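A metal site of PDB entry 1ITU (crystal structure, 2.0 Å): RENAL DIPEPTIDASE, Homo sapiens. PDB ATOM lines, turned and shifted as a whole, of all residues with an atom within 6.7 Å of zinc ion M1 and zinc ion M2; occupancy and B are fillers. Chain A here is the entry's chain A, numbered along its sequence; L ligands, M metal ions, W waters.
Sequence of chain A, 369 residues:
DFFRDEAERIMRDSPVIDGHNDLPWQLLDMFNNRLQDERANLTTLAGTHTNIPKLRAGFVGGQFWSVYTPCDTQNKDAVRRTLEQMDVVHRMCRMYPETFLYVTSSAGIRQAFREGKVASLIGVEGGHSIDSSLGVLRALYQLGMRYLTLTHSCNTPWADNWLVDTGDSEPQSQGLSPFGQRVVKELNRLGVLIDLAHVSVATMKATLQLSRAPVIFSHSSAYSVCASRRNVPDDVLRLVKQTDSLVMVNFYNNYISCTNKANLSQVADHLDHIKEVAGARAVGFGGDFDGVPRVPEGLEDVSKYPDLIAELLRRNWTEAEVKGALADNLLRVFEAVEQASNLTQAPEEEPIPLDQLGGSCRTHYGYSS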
ATOM      1  N   HIS A  20     -26.321 -30.108  24.242  1.00  0.00           N
ATOM      2  CA  HIS A  20     -25.788 -28.770  24.484  1.00  0.00           C
ATOM      3  C   HIS A  20     -26.175 -27.693  23.477  1.00  0.00           C
ATOM      4  O   HIS A  20     -25.670 -27.662  22.367  1.00  0.00           O
ATOM      5  CB  HIS A  20     -24.275 -28.823  24.577  1.00  0.00           C
ATOM      6  CG  HIS A  20     -23.667 -27.614  25.207  1.00  0.00           C
ATOM      7  ND1 HIS A  20     -23.513 -27.460  26.574  1.00  0.00           N
ATOM      8  CD2 HIS A  20     -23.175 -26.480  24.649  1.00  0.00           C
ATOM      9  CE1 HIS A  20     -22.938 -26.276  26.790  1.00  0.00           C
ATOM     10  NE2 HIS A  20     -22.710 -25.644  25.655  1.00  0.00           N
ATOM     11  N   ASN A  21     -27.014 -26.757  23.913  1.00  0.00           N
ATOM     12  CA  ASN A  21     -27.426 -25.658  23.067  1.00  0.00           C
ATOM     13  C   ASN A  21     -27.287 -24.348  23.860  1.00  0.00           C
ATOM     14  O   ASN A  21     -27.842 -24.224  24.957  1.00  0.00           O
ATOM     15  CB  ASN A  21     -28.869 -25.871  22.618  1.00  0.00           C
ATOM     16  CG  ASN A  21     -29.347 -24.792  21.684  1.00  0.00           C
ATOM     17  OD1 ASN A  21     -29.355 -23.615  22.033  1.00  0.00           O
ATOM     18  ND2 ASN A  21     -29.750 -25.190  20.487  1.00  0.00           N
ATOM     19  N   ASP A  22     -26.511 -23.411  23.331  1.00  0.00           N
ATOM     20  CA  ASP A  22     -26.274 -22.124  23.987  1.00  0.00           C
ATOM     21  C   ASP A  22     -27.261 -20.989  23.695  1.00  0.00           C
ATOM     22  O   ASP A  22     -26.865 -19.817  23.684  1.00  0.00           O
ATOM     23  CB  ASP A  22     -24.854 -21.626  23.704  1.00  0.00           C
ATOM     24  CG  ASP A  22     -23.825 -22.249  24.623  1.00  0.00           C
ATOM     25  OD1 ASP A  22     -22.847 -22.800  24.100  1.00  0.00           O
ATOM     26  OD2 ASP A  22     -23.977 -22.151  25.864  1.00  0.00           O
ATOM     27  N   SER A  66     -27.878 -24.953  27.748  1.00  0.00           N
ATOM     28  CA  SER A  66     -26.677 -24.545  28.445  1.00  0.00           C
ATOM     29  C   SER A  66     -26.830 -23.259  29.252  1.00  0.00           C
ATOM     30  O   SER A  66     -27.352 -22.246  28.756  1.00  0.00           O
ATOM     31  CB  SER A  66     -25.526 -24.383  27.449  1.00  0.00           C
ATOM     32  OG  SER A  66     -24.383 -23.854  28.093  1.00  0.00           O
ATOM     33  N   TYR A  68     -24.456 -21.025  30.701  1.00  0.00           N
ATOM     34  CA  TYR A  68     -23.056 -20.699  30.600  1.00  0.00           C
ATOM     35  C   TYR A  68     -22.732 -19.254  30.966  1.00  0.00           C
ATOM     36  O   TYR A  68     -23.437 -18.328  30.570  1.00  0.00           O
ATOM     37  CB  TYR A  68     -22.606 -21.013  29.170  1.00  0.00           C
ATOM     38  CG  TYR A  68     -21.389 -20.276  28.717  1.00  0.00           C
ATOM     39  CD1 TYR A  68     -21.501 -19.154  27.896  1.00  0.00           C
ATOM     40  CD2 TYR A  68     -20.113 -20.690  29.096  1.00  0.00           C
ATOM     41  CE1 TYR A  68     -20.369 -18.451  27.471  1.00  0.00           C
ATOM     42  CE2 TYR A  68     -18.980 -20.002  28.681  1.00  0.00           C
ATOM     43  CZ  TYR A  68     -19.113 -18.885  27.864  1.00  0.00           C
ATOM     44  OH  TYR A  68     -17.991 -18.195  27.462  1.00  0.00           O
ATOM     45  N   GLU A 125     -22.518 -25.142  32.254  1.00  0.00           N
ATOM     46  CA  GLU A 125     -21.231 -25.199  31.567  1.00  0.00           C
ATOM     47  C   GLU A 125     -20.035 -24.527  32.215  1.00  0.00           C
ATOM     48  O   GLU A 125     -19.659 -23.411  31.857  1.00  0.00           O
ATOM     49  CB  GLU A 125     -21.381 -24.740  30.111  1.00  0.00           C
ATOM     50  CG  GLU A 125     -20.124 -25.041  29.319  1.00  0.00           C
ATOM     51  CD  GLU A 125     -20.173 -24.707  27.855  1.00  0.00           C
ATOM     52  OE1 GLU A 125     -20.949 -23.829  27.432  1.00  0.00           O
ATOM     53  OE2 GLU A 125     -19.391 -25.326  27.117  1.00  0.00           O
ATOM     54  N   THR A 149     -20.592 -29.337  33.477  1.00  0.00           N
ATOM     55  CA  THR A 149     -19.392 -29.432  32.655  1.00  0.00           C
ATOM     56  C   THR A 149     -18.314 -28.994  33.659  1.00  0.00           C
ATOM     57  O   THR A 149     -18.325 -27.840  34.099  1.00  0.00           O
ATOM     58  CB  THR A 149     -19.449 -28.426  31.498  1.00  0.00           C
ATOM     59  OG1 THR A 149     -20.727 -28.520  30.852  1.00  0.00           O
ATOM     60  CG2 THR A 149     -18.347 -28.700  30.496  1.00  0.00           C
ATOM     61  N   HIS A 152     -14.898 -24.956  31.803  1.00  0.00           N
ATOM     62  CA  HIS A 152     -15.225 -24.436  30.503  1.00  0.00           C
ATOM     63  C   HIS A 152     -13.792 -24.320  29.954  1.00  0.00           C
ATOM     64  O   HIS A 152     -13.001 -25.239  30.146  1.00  0.00           O
ATOM     65  CB  HIS A 152     -15.923 -23.068  30.524  1.00  0.00           C
ATOM     66  CG  HIS A 152     -16.270 -22.588  29.155  1.00  0.00           C
ATOM     67  ND1 HIS A 152     -15.652 -21.503  28.566  1.00  0.00           N
ATOM     68  CD2 HIS A 152     -17.070 -23.115  28.197  1.00  0.00           C
ATOM     69  CE1 HIS A 152     -16.051 -21.396  27.307  1.00  0.00           C
ATOM     70  NE2 HIS A 152     -16.915 -22.361  27.064  1.00  0.00           N
ATOM     71  N   SER A 153     -13.447 -23.197  29.337  1.00  0.00           N
ATOM     72  CA  SER A 153     -12.099 -23.022  28.800  1.00  0.00           C
ATOM     73  C   SER A 153     -11.148 -22.283  29.742  1.00  0.00           C
ATOM     74  O   SER A 153     -10.391 -21.388  29.340  1.00  0.00           O
ATOM     75  CB  SER A 153     -12.146 -22.383  27.420  1.00  0.00           C
ATOM     76  OG  SER A 153     -12.873 -23.219  26.546  1.00  0.00           O
ATOM     77  N   ALA A 197     -16.951 -32.317  28.610  1.00  0.00           N
ATOM     78  CA  ALA A 197     -16.654 -31.409  27.512  1.00  0.00           C
ATOM     79  C   ALA A 197     -15.750 -30.325  28.120  1.00  0.00           C
ATOM     80  O   ALA A 197     -15.847 -30.019  29.315  1.00  0.00           O
ATOM     81  CB  ALA A 197     -17.948 -30.769  26.982  1.00  0.00           C
ATOM     82  N   HIS A 198     -14.801 -29.823  27.318  1.00  0.00           N
ATOM     83  CA  HIS A 198     -13.892 -28.759  27.740  1.00  0.00           C
ATOM     84  C   HIS A 198     -12.811 -29.068  28.763  1.00  0.00           C
ATOM     85  O   HIS A 198     -12.075 -28.169  29.146  1.00  0.00           O
ATOM     86  CB  HIS A 198     -14.679 -27.545  28.268  1.00  0.00           C
ATOM     87  CG  HIS A 198     -15.369 -26.746  27.217  1.00  0.00           C
ATOM     88  ND1 HIS A 198     -14.773 -25.707  26.528  1.00  0.00           N
ATOM     89  CD2 HIS A 198     -16.645 -26.814  26.756  1.00  0.00           C
ATOM     90  CE1 HIS A 198     -15.691 -25.198  25.701  1.00  0.00           C
ATOM     91  NE2 HIS A 198     -16.835 -25.838  25.793  1.00  0.00           N
ATOM     92  N   SER A 218     -20.995 -33.600  26.750  1.00  0.00           N
ATOM     93  CA  SER A 218     -22.216 -32.990  26.203  1.00  0.00           C
ATOM     94  C   SER A 218     -22.091 -32.421  24.812  1.00  0.00           C
ATOM     95  O   SER A 218     -23.093 -32.239  24.124  1.00  0.00           O
ATOM     96  CB  SER A 218     -22.759 -31.911  27.152  1.00  0.00           C
ATOM     97  OG  SER A 218     -21.963 -30.741  27.100  1.00  0.00           O
ATOM     98  N   HIS A 219     -20.872 -32.070  24.424  1.00  0.00           N
ATOM     99  CA  HIS A 219     -20.596 -31.540  23.100  1.00  0.00           C
ATOM    100  C   HIS A 219     -19.096 -31.619  22.744  1.00  0.00           C
ATOM    101  O   HIS A 219     -18.358 -30.629  22.780  1.00  0.00           O
ATOM    102  CB  HIS A 219     -21.188 -30.110  22.925  1.00  0.00           C
ATOM    103  CG  HIS A 219     -20.688 -29.100  23.900  1.00  0.00           C
ATOM    104  ND1 HIS A 219     -20.763 -29.241  25.276  1.00  0.00           N
ATOM    105  CD2 HIS A 219     -20.060 -27.923  23.692  1.00  0.00           C
ATOM    106  CE1 HIS A 219     -20.193 -28.176  25.837  1.00  0.00           C
ATOM    107  NE2 HIS A 219     -19.749 -27.344  24.908  1.00  0.00           N
ATOM    108  N   ARG A 230     -10.420 -30.254  22.008  1.00  0.00           N
ATOM    109  CA  ARG A 230     -11.775 -30.157  22.506  1.00  0.00           C
ATOM    110  C   ARG A 230     -12.452 -31.484  22.175  1.00  0.00           C
ATOM    111  O   ARG A 230     -13.585 -31.746  22.577  1.00  0.00           O
ATOM    112  CB  ARG A 230     -12.520 -28.988  21.863  1.00  0.00           C
ATOM    113  CG  ARG A 230     -12.476 -27.725  22.706  1.00  0.00           C
ATOM    114  CD  ARG A 230     -13.328 -27.903  23.961  1.00  0.00           C
ATOM    115  NE  ARG A 230     -14.751 -27.737  23.667  1.00  0.00           N
ATOM    116  CZ  ARG A 230     -15.667 -28.687  23.755  1.00  0.00           C
ATOM    117  NH1 ARG A 230     -16.938 -28.417  23.471  1.00  0.00           N
ATOM    118  NH2 ARG A 230     -15.320 -29.921  24.107  1.00  0.00           N
ATOM    119  N   ASN A 250     -20.377 -32.731  18.873  1.00  0.00           N
ATOM    120  CA  ASN A 250     -20.395 -31.280  18.640  1.00  0.00           C
ATOM    121  C   ASN A 250     -20.347 -31.027  17.130  1.00  0.00           C
ATOM    122  O   ASN A 250     -19.567 -31.667  16.423  1.00  0.00           O
ATOM    123  CB  ASN A 250     -19.166 -30.683  19.339  1.00  0.00           C
ATOM    124  CG  ASN A 250     -19.178 -29.160  19.384  1.00  0.00           C
ATOM    125  OD1 ASN A 250     -19.652 -28.494  18.473  1.00  0.00           O
ATOM    126  ND2 ASN A 250     -18.583 -28.610  20.451  1.00  0.00           N
ATOM    127  N   TYR A 255     -14.024 -28.296  14.895  1.00  0.00           N
ATOM    128  CA  TYR A 255     -13.828 -29.491  15.704  1.00  0.00           C
ATOM    129  C   TYR A 255     -14.183 -30.726  14.861  1.00  0.00           C
ATOM    130  O   TYR A 255     -13.875 -31.863  15.216  1.00  0.00           O
ATOM    131  CB  TYR A 255     -14.706 -29.475  16.973  1.00  0.00           C
ATOM    132  CG  TYR A 255     -14.393 -28.351  17.944  1.00  0.00           C
ATOM    133  CD1 TYR A 255     -13.241 -27.569  17.816  1.00  0.00           C
ATOM    134  CD2 TYR A 255     -15.270 -28.068  18.998  1.00  0.00           C
ATOM    135  CE1 TYR A 255     -12.971 -26.525  18.701  1.00  0.00           C
ATOM    136  CE2 TYR A 255     -15.011 -27.008  19.886  1.00  0.00           C
ATOM    137  CZ  TYR A 255     -13.870 -26.253  19.728  1.00  0.00           C
ATOM    138  OH  TYR A 255     -13.647 -25.203  20.594  1.00  0.00           O
ATOM    139  N   ASP A 288     -23.933 -28.020  19.841  1.00  0.00           N
ATOM    140  CA  ASP A 288     -23.314 -26.752  20.234  1.00  0.00           C
ATOM    141  C   ASP A 288     -23.906 -25.583  19.432  1.00  0.00           C
ATOM    142  O   ASP A 288     -23.259 -24.551  19.245  1.00  0.00           O
ATOM    143  CB  ASP A 288     -21.782 -26.824  20.076  1.00  0.00           C
ATOM    144  CG  ASP A 288     -21.039 -25.869  20.993  1.00  0.00           C
ATOM    145  OD1 ASP A 288     -21.696 -25.203  21.838  1.00  0.00           O
ATOM    146  OD2 ASP A 288     -19.806 -25.787  20.889  1.00  0.00           O
ATOM    147  N   GLY A 291     -23.803 -21.656  20.177  1.00  0.00           N
ATOM    148  CA  GLY A 291     -22.620 -21.518  20.990  1.00  0.00           C
ATOM    149  C   GLY A 291     -21.402 -21.444  20.099  1.00  0.00           C
ATOM    150  O   GLY A 291     -20.295 -21.214  20.574  1.00  0.00           O
HETATM  151  C1  LIG L   1     -19.800 -21.072  25.200  1.00  0.00           C
HETATM  152  C2  LIG L   1     -19.547 -21.477  23.780  1.00  0.00           C
HETATM  153  C3  LIG L   1     -19.339 -20.055  24.192  1.00  0.00           C
HETATM  154  C4  LIG L   1     -17.920 -19.542  24.300  1.00  0.00           C
HETATM  155  C5  LIG L   1     -20.326 -19.031  23.700  1.00  0.00           C
HETATM  156  C6  LIG L   1     -18.405 -22.321  23.474  1.00  0.00           C
HETATM  157  N1  LIG L   1     -18.331 -22.829  22.184  1.00  0.00           N
HETATM  158  C7  LIG L   1     -17.322 -23.635  21.755  1.00  0.00           C
HETATM  159  C8  LIG L   1     -16.605 -23.316  20.670  1.00  0.00           C
HETATM  160  O1  LIG L   1     -17.558 -22.580  24.317  1.00  0.00           O
HETATM  161  C9  LIG L   1     -16.990 -24.937  22.478  1.00  0.00           C
HETATM  162  O2  LIG L   1     -15.814 -25.293  22.584  1.00  0.00           O
HETATM  163  O3  LIG L   1     -17.885 -25.618  22.941  1.00  0.00           O
HETATM  164  C10 LIG L   1     -16.809 -22.077  19.865  1.00  0.00           C
HETATM  165  C11 LIG L   1     -15.579 -21.201  20.000  1.00  0.00           C
HETATM  166  C12 LIG L   1     -15.608 -20.093  18.944  1.00  0.00           C
HETATM  167 ZN    ZN M   1     -21.731 -23.894  25.422  1.00  0.00          ZN
HETATM  168 ZN    ZN M   2     -18.864 -25.453  24.989  1.00  0.00          ZN
HETATM  169  O   HOH W   1     -20.294 -24.403  23.809  1.00  0.00           O
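An oxygen (O2) of the ligand lies within salt-bridge range of the guanidinium group (NE) of Arg 230 (2.9 Å). O1 of the ligand is in hydrogen-bond range of NE2 of His 152, 2.8 Å away. O of Gly 291 is in hydrogen-bond range of N1 of the ligand (3.0 Å). The side-chain hydroxyl of Tyr 255 is in hydrogen-bond range of an oxygen (O2) of the ligand (2.9 Å).
A ring nitrogen (NE2) of His 20 sits close to the side-chain hydroxyl (OG) of Ser 66, 3.5 Å away. The side-chain carboxylate of Asp 22 lies within hydrogen-bond range of the side-chain hydroxyl of Ser 66 (2.8 Å). The backbone carbonyl oxygen (O) of His 219 is in hydrogen-bond range of the guanidinium group (NH1) of Arg 230 (2.7 Å). The side-chain hydroxyl of Ser 218 sits at hydrogen-bond distance from a ring nitrogen (ND1) of His 219 (2.6 Å). NH1 of Arg 230 lies close to NE2 of His 198, at 3.5 Å. A ring nitrogen (ND1) of His 198 lies within hydrogen-bond range of the side-chain hydroxyl of Ser 153 (3.1 Å). The backbone carbonyl oxygen (O) of Asn 21 sits at hydrogen-bond distance from the backbone NH (N) of Ser 66 (2.9 Å). The side-chain amide nitrogen (ND2) of Asn 250 sits close to the guanidinium group (NH1) of Arg 230 (3.4 Å).
Residues that only touch zinc ion M1: Ser 66 (3.8 Å) and Asp 288 (3.8 Å). Of the 18 residues printed, 5 come within 4 Å of zinc ion M1. The nearest printed residue that does not touch zinc ion M1 is His 219 (4.01 Å).
Arg 230 touches zinc ion M2. Five residues have an atom within 4 Å of zinc ion M2: His 20, Glu 125, His 198, His 219 and Arg 230.
Zinc ion M1 is bound by NE2 of His 20 (2.0 Å). OD1 of Asp 22 binds zinc ion M1. Zinc ion M1 is bound by OE1 of Glu 125, at 2.2 Å. Water W1 binds zinc ion M1.
Zinc ion M2 is bound by NE2 of His 219, water W1, OE2 of Glu 125, NE2 of His 198 and O3 of the ligand.
Water W1 lies within hydrogen-bond range of OD1 of Asp 288 (2.5 Å) and N1 of the ligand (3.0 Å).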
